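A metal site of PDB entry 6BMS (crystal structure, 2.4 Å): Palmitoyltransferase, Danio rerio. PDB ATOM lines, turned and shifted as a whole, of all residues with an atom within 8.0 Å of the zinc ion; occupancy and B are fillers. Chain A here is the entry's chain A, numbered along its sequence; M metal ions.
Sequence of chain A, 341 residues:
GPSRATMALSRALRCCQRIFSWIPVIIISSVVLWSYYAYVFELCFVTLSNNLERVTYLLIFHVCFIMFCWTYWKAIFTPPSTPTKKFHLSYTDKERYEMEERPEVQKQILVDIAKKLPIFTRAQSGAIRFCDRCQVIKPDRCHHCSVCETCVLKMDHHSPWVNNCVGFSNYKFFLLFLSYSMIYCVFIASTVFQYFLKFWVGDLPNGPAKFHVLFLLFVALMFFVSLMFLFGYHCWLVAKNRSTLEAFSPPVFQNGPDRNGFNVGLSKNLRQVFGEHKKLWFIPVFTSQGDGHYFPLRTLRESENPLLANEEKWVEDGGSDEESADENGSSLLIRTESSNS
Merely in contact with the zinc ion: Thr 150 (3.9 Å).
Five residues have an atom within 4 Å of the zinc ion: Cys 131, Cys 134, His 144, Thr 150 and Cys 151.
Along chain A the residues within 4 Å of the zinc ion span positions 131 to 151.
The nearest printed residue that does not touch the zinc ion is Arg 133 (4.9 Å).
The zinc ion is bound by ND1 of His 144 (2.2 Å), SG of Cys 131 (2.4 Å), SG of Cys 151 (2.4 Å) and SG of Cys 134 (2.5 Å).
The backbone carbonyl oxygen (O) of Thr 150 sits close to a ring nitrogen (ND1) of His 144.
The backbone NH of Arg 133 sits close to the side-chain sulfur of Cys 131 (3.6 Å).
The backbone carbonyl oxygen (O) of Val 136 lies within hydrogen-bond range of the backbone NH (N) of Cys 131, 3.0 Å away.
O of Thr 150 sits at hydrogen-bond distance from N of Cys 145.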
ATOM      1  N   PRO A  83      23.745 -17.646 -11.407  1.00  0.00           N
ATOM      2  CA  PRO A  83      24.124 -18.569 -12.476  1.00  0.00           C
ATOM      3  C   PRO A  83      24.342 -17.856 -13.807  1.00  0.00           C
ATOM      4  O   PRO A  83      23.655 -16.887 -14.129  1.00  0.00           O
ATOM      5  CB  PRO A  83      22.937 -19.535 -12.544  1.00  0.00           C
ATOM      6  CG  PRO A  83      22.343 -19.503 -11.185  1.00  0.00           C
ATOM      7  CD  PRO A  83      22.533 -18.093 -10.698  1.00  0.00           C
ATOM      8  N   HIS A  88      20.928 -20.752 -17.942  1.00  0.00           N
ATOM      9  CA  HIS A  88      19.621 -20.162 -18.127  1.00  0.00           C
ATOM     10  C   HIS A  88      18.913 -20.785 -19.321  1.00  0.00           C
ATOM     11  O   HIS A  88      19.533 -21.153 -20.323  1.00  0.00           O
ATOM     12  CB  HIS A  88      19.732 -18.656 -18.341  1.00  0.00           C
ATOM     13  CG  HIS A  88      19.864 -17.868 -17.074  1.00  0.00           C
ATOM     14  ND1 HIS A  88      21.036 -17.819 -16.351  1.00  0.00           N
ATOM     15  CD2 HIS A  88      18.984 -17.085 -16.418  1.00  0.00           C
ATOM     16  CE1 HIS A  88      20.872 -17.049 -15.294  1.00  0.00           C
ATOM     17  NE2 HIS A  88      19.626 -16.590 -15.305  1.00  0.00           N
ATOM     18  N   PHE A 130      15.220 -27.009 -10.936  1.00  0.00           N
ATOM     19  CA  PHE A 130      14.873 -25.949 -11.874  1.00  0.00           C
ATOM     20  C   PHE A 130      14.070 -24.880 -11.162  1.00  0.00           C
ATOM     21  O   PHE A 130      13.191 -25.187 -10.352  1.00  0.00           O
ATOM     22  CB  PHE A 130      14.070 -26.504 -13.057  1.00  0.00           C
ATOM     23  CG  PHE A 130      13.711 -25.461 -14.084  1.00  0.00           C
ATOM     24  CD1 PHE A 130      14.667 -24.976 -14.966  1.00  0.00           C
ATOM     25  CD2 PHE A 130      12.411 -24.981 -14.182  1.00  0.00           C
ATOM     26  CE1 PHE A 130      14.332 -24.023 -15.916  1.00  0.00           C
ATOM     27  CE2 PHE A 130      12.075 -24.028 -15.131  1.00  0.00           C
ATOM     28  CZ  PHE A 130      13.029 -23.544 -15.999  1.00  0.00           C
ATOM     29  N   CYS A 131      14.375 -23.625 -11.476  1.00  0.00           N
ATOM     30  CA  CYS A 131      13.715 -22.484 -10.867  1.00  0.00           C
ATOM     31  C   CYS A 131      12.796 -21.837 -11.900  1.00  0.00           C
ATOM     32  O   CYS A 131      13.270 -21.291 -12.901  1.00  0.00           O
ATOM     33  CB  CYS A 131      14.730 -21.477 -10.342  1.00  0.00           C
ATOM     34  SG  CYS A 131      13.984 -19.993  -9.670  1.00  0.00           S
ATOM     35  N   ASP A 132      11.490 -21.871 -11.647  1.00  0.00           N
ATOM     36  CA  ASP A 132      10.528 -21.283 -12.575  1.00  0.00           C
ATOM     37  C   ASP A 132      10.689 -19.771 -12.660  1.00  0.00           C
ATOM     38  O   ASP A 132      10.445 -19.180 -13.723  1.00  0.00           O
ATOM     39  CB  ASP A 132       9.105 -21.639 -12.150  1.00  0.00           C
ATOM     40  CG  ASP A 132       8.769 -23.094 -12.375  1.00  0.00           C
ATOM     41  OD1 ASP A 132       9.289 -23.690 -13.340  1.00  0.00           O
ATOM     42  OD2 ASP A 132       7.972 -23.643 -11.581  1.00  0.00           O
ATOM     43  N   ARG A 133      11.080 -19.120 -11.569  1.00  0.00           N
ATOM     44  CA  ARG A 133      11.112 -17.661 -11.547  1.00  0.00           C
ATOM     45  C   ARG A 133      12.316 -17.121 -12.303  1.00  0.00           C
ATOM     46  O   ARG A 133      12.194 -16.168 -13.077  1.00  0.00           O
ATOM     47  CB  ARG A 133      11.106 -17.159 -10.095  1.00  0.00           C
ATOM     48  CG  ARG A 133       9.765 -17.325  -9.411  1.00  0.00           C
ATOM     49  CD  ARG A 133       9.890 -17.316  -7.895  1.00  0.00           C
ATOM     50  NE  ARG A 133       8.848 -18.132  -7.259  1.00  0.00           N
ATOM     51  CZ  ARG A 133       9.042 -18.884  -6.183  1.00  0.00           C
ATOM     52  NH1 ARG A 133      10.240 -18.944  -5.620  1.00  0.00           N
ATOM     53  NH2 ARG A 133       8.041 -19.583  -5.678  1.00  0.00           N
ATOM     54  N   CYS A 134      13.491 -17.705 -12.094  1.00  0.00           N
ATOM     55  CA  CYS A 134      14.703 -17.274 -12.776  1.00  0.00           C
ATOM     56  C   CYS A 134      14.921 -17.960 -14.113  1.00  0.00           C
ATOM     57  O   CYS A 134      15.791 -17.531 -14.882  1.00  0.00           O
ATOM     58  CB  CYS A 134      15.929 -17.514 -11.881  1.00  0.00           C
ATOM     59  SG  CYS A 134      15.926 -16.555 -10.346  1.00  0.00           S
ATOM     60  N   GLN A 135      14.146 -19.003 -14.432  1.00  0.00           N
ATOM     61  CA  GLN A 135      14.371 -19.836 -15.619  1.00  0.00           C
ATOM     62  C   GLN A 135      15.792 -20.384 -15.622  1.00  0.00           C
ATOM     63  O   GLN A 135      16.522 -20.264 -16.608  1.00  0.00           O
ATOM     64  CB  GLN A 135      14.068 -19.061 -16.903  1.00  0.00           C
ATOM     65  CG  GLN A 135      12.598 -18.797 -17.131  1.00  0.00           C
ATOM     66  CD  GLN A 135      11.808 -20.059 -17.370  1.00  0.00           C
ATOM     67  OE1 GLN A 135      12.029 -20.778 -18.351  1.00  0.00           O
ATOM     68  NE2 GLN A 135      10.868 -20.348 -16.475  1.00  0.00           N
ATOM     69  N   VAL A 136      16.181 -20.992 -14.509  1.00  0.00           N
ATOM     70  CA  VAL A 136      17.558 -21.386 -14.259  1.00  0.00           C
ATOM     71  C   VAL A 136      17.596 -22.880 -13.950  1.00  0.00           C
ATOM     72  O   VAL A 136      16.845 -23.365 -13.095  1.00  0.00           O
ATOM     73  CB  VAL A 136      18.168 -20.585 -13.098  1.00  0.00           C
ATOM     74  CG1 VAL A 136      19.246 -21.387 -12.379  1.00  0.00           C
ATOM     75  CG2 VAL A 136      18.741 -19.273 -13.605  1.00  0.00           C
ATOM     76  N   LYS A 138      19.373 -24.948 -11.900  1.00  0.00           N
ATOM     77  CA  LYS A 138      20.167 -24.617 -10.717  1.00  0.00           C
ATOM     78  C   LYS A 138      21.488 -25.369 -10.718  1.00  0.00           C
ATOM     79  O   LYS A 138      21.489 -26.611 -10.809  1.00  0.00           O
ATOM     80  CB  LYS A 138      19.382 -24.932  -9.449  1.00  0.00           C
ATOM     81  CG  LYS A 138      18.206 -24.030  -9.182  1.00  0.00           C
ATOM     82  CD  LYS A 138      17.449 -24.492  -7.954  1.00  0.00           C
ATOM     83  CE  LYS A 138      16.141 -23.745  -7.772  1.00  0.00           C
ATOM     84  NZ  LYS A 138      15.310 -24.336  -6.698  1.00  0.00           N
ATOM     85  N   CYS A 142      23.355 -24.169  -5.521  1.00  0.00           N
ATOM     86  CA  CYS A 142      22.625 -22.941  -5.770  1.00  0.00           C
ATOM     87  C   CYS A 142      21.166 -23.101  -5.340  1.00  0.00           C
ATOM     88  O   CYS A 142      20.554 -24.135  -5.583  1.00  0.00           O
ATOM     89  CB  CYS A 142      22.678 -22.561  -7.252  1.00  0.00           C
ATOM     90  SG  CYS A 142      21.581 -21.208  -7.728  1.00  0.00           S
ATOM     91  N   HIS A 143      20.628 -22.080  -4.683  1.00  0.00           N
ATOM     92  CA  HIS A 143      19.239 -22.132  -4.222  1.00  0.00           C
ATOM     93  C   HIS A 143      18.556 -20.802  -4.487  1.00  0.00           C
ATOM     94  O   HIS A 143      19.218 -19.771  -4.602  1.00  0.00           O
ATOM     95  CB  HIS A 143      19.147 -22.494  -2.731  1.00  0.00           C
ATOM     96  CG  HIS A 143      19.772 -23.812  -2.388  1.00  0.00           C
ATOM     97  ND1 HIS A 143      19.034 -24.954  -2.191  1.00  0.00           N
ATOM     98  CD2 HIS A 143      21.065 -24.163  -2.213  1.00  0.00           C
ATOM     99  CE1 HIS A 143      19.844 -25.961  -1.910  1.00  0.00           C
ATOM    100  NE2 HIS A 143      21.082 -25.501  -1.913  1.00  0.00           N
ATOM    101  N   HIS A 144      17.233 -20.836  -4.580  1.00  0.00           N
ATOM    102  CA  HIS A 144      16.481 -19.615  -4.819  1.00  0.00           C
ATOM    103  C   HIS A 144      16.160 -18.929  -3.497  1.00  0.00           C
ATOM    104  O   HIS A 144      15.677 -19.558  -2.552  1.00  0.00           O
ATOM    105  CB  HIS A 144      15.186 -19.912  -5.581  1.00  0.00           C
ATOM    106  CG  HIS A 144      14.476 -18.690  -6.071  1.00  0.00           C
ATOM    107  ND1 HIS A 144      15.104 -17.697  -6.802  1.00  0.00           N
ATOM    108  CD2 HIS A 144      13.189 -18.290  -5.920  1.00  0.00           C
ATOM    109  CE1 HIS A 144      14.230 -16.753  -7.096  1.00  0.00           C
ATOM    110  NE2 HIS A 144      13.064 -17.074  -6.566  1.00  0.00           N
ATOM    111  N   CYS A 145      16.462 -17.636  -3.422  1.00  0.00           N
ATOM    112  CA  CYS A 145      16.079 -16.812  -2.280  1.00  0.00           C
ATOM    113  C   CYS A 145      14.870 -15.970  -2.666  1.00  0.00           C
ATOM    114  O   CYS A 145      14.954 -15.140  -3.581  1.00  0.00           O
ATOM    115  CB  CYS A 145      17.218 -15.901  -1.829  1.00  0.00           C
ATOM    116  SG  CYS A 145      16.726 -14.830  -0.461  1.00  0.00           S
ATOM    117  N   SER A 146      13.759 -16.181  -1.957  1.00  0.00           N
ATOM    118  CA  SER A 146      12.547 -15.423  -2.240  1.00  0.00           C
ATOM    119  C   SER A 146      12.630 -13.992  -1.718  1.00  0.00           C
ATOM    120  O   SER A 146      11.883 -13.127  -2.197  1.00  0.00           O
ATOM    121  CB  SER A 146      11.329 -16.127  -1.625  1.00  0.00           C
ATOM    122  OG  SER A 146      11.400 -16.095  -0.208  1.00  0.00           O
ATOM    123  N   GLU A 149      14.846 -12.735  -4.150  1.00  0.00           N
ATOM    124  CA  GLU A 149      14.085 -13.101  -5.345  1.00  0.00           C
ATOM    125  C   GLU A 149      15.002 -13.507  -6.483  1.00  0.00           C
ATOM    126  O   GLU A 149      14.761 -13.201  -7.655  1.00  0.00           O
ATOM    127  CB  GLU A 149      13.169 -11.953  -5.798  1.00  0.00           C
ATOM    128  CG  GLU A 149      12.293 -11.366  -4.708  1.00  0.00           C
ATOM    129  CD  GLU A 149      11.658 -10.064  -5.154  1.00  0.00           C
ATOM    130  OE1 GLU A 149      10.477 -10.082  -5.554  1.00  0.00           O
ATOM    131  OE2 GLU A 149      12.338  -9.015  -5.093  1.00  0.00           O
ATOM    132  N   THR A 150      16.070 -14.234  -6.148  1.00  0.00           N
ATOM    133  CA  THR A 150      16.998 -14.667  -7.186  1.00  0.00           C
ATOM    134  C   THR A 150      17.692 -15.945  -6.752  1.00  0.00           C
ATOM    135  O   THR A 150      17.846 -16.225  -5.555  1.00  0.00           O
ATOM    136  CB  THR A 150      18.045 -13.596  -7.527  1.00  0.00           C
ATOM    137  OG1 THR A 150      18.833 -14.055  -8.630  1.00  0.00           O
ATOM    138  CG2 THR A 150      18.954 -13.342  -6.338  1.00  0.00           C
ATOM    139  N   CYS A 151      18.091 -16.730  -7.738  1.00  0.00           N
ATOM    140  CA  CYS A 151      18.953 -17.868  -7.486  1.00  0.00           C
ATOM    141  C   CYS A 151      20.335 -17.380  -7.072  1.00  0.00           C
ATOM    142  O   CYS A 151      20.895 -16.454  -7.659  1.00  0.00           O
ATOM    143  CB  CYS A 151      19.026 -18.767  -8.721  1.00  0.00           C
ATOM    144  SG  CYS A 151      17.627 -19.903  -8.866  1.00  0.00           S
ATOM    145  N   VAL A 152      20.872 -18.018  -6.038  1.00  0.00           N
ATOM    146  CA  VAL A 152      22.094 -17.602  -5.358  1.00  0.00           C
ATOM    147  C   VAL A 152      23.027 -18.798  -5.306  1.00  0.00           C
ATOM    148  O   VAL A 152      22.622 -19.898  -4.906  1.00  0.00           O
ATOM    149  CB  VAL A 152      21.798 -17.065  -3.933  1.00  0.00           C
ATOM    150  CG1 VAL A 152      23.082 -16.852  -3.155  1.00  0.00           C
ATOM    151  CG2 VAL A 152      20.957 -15.783  -3.995  1.00  0.00           C
ATOM    152  N   MET A 155      24.359 -20.718  -1.783  1.00  0.00           N
ATOM    153  CA  MET A 155      23.635 -19.946  -0.782  1.00  0.00           C
ATOM    154  C   MET A 155      23.740 -20.624   0.571  1.00  0.00           C
ATOM    155  O   MET A 155      23.263 -21.750   0.752  1.00  0.00           O
ATOM    156  CB  MET A 155      22.177 -19.779  -1.171  1.00  0.00           C
ATOM    157  CG  MET A 155      21.415 -18.892  -0.204  1.00  0.00           C
ATOM    158  SD  MET A 155      19.665 -19.301  -0.125  1.00  0.00           S
ATOM    159  CE  MET A 155      19.162 -18.734  -1.745  1.00  0.00           C
HETATM  160 ZN    ZN M   1      15.653 -18.523  -8.807  1.00  0.00          ZN
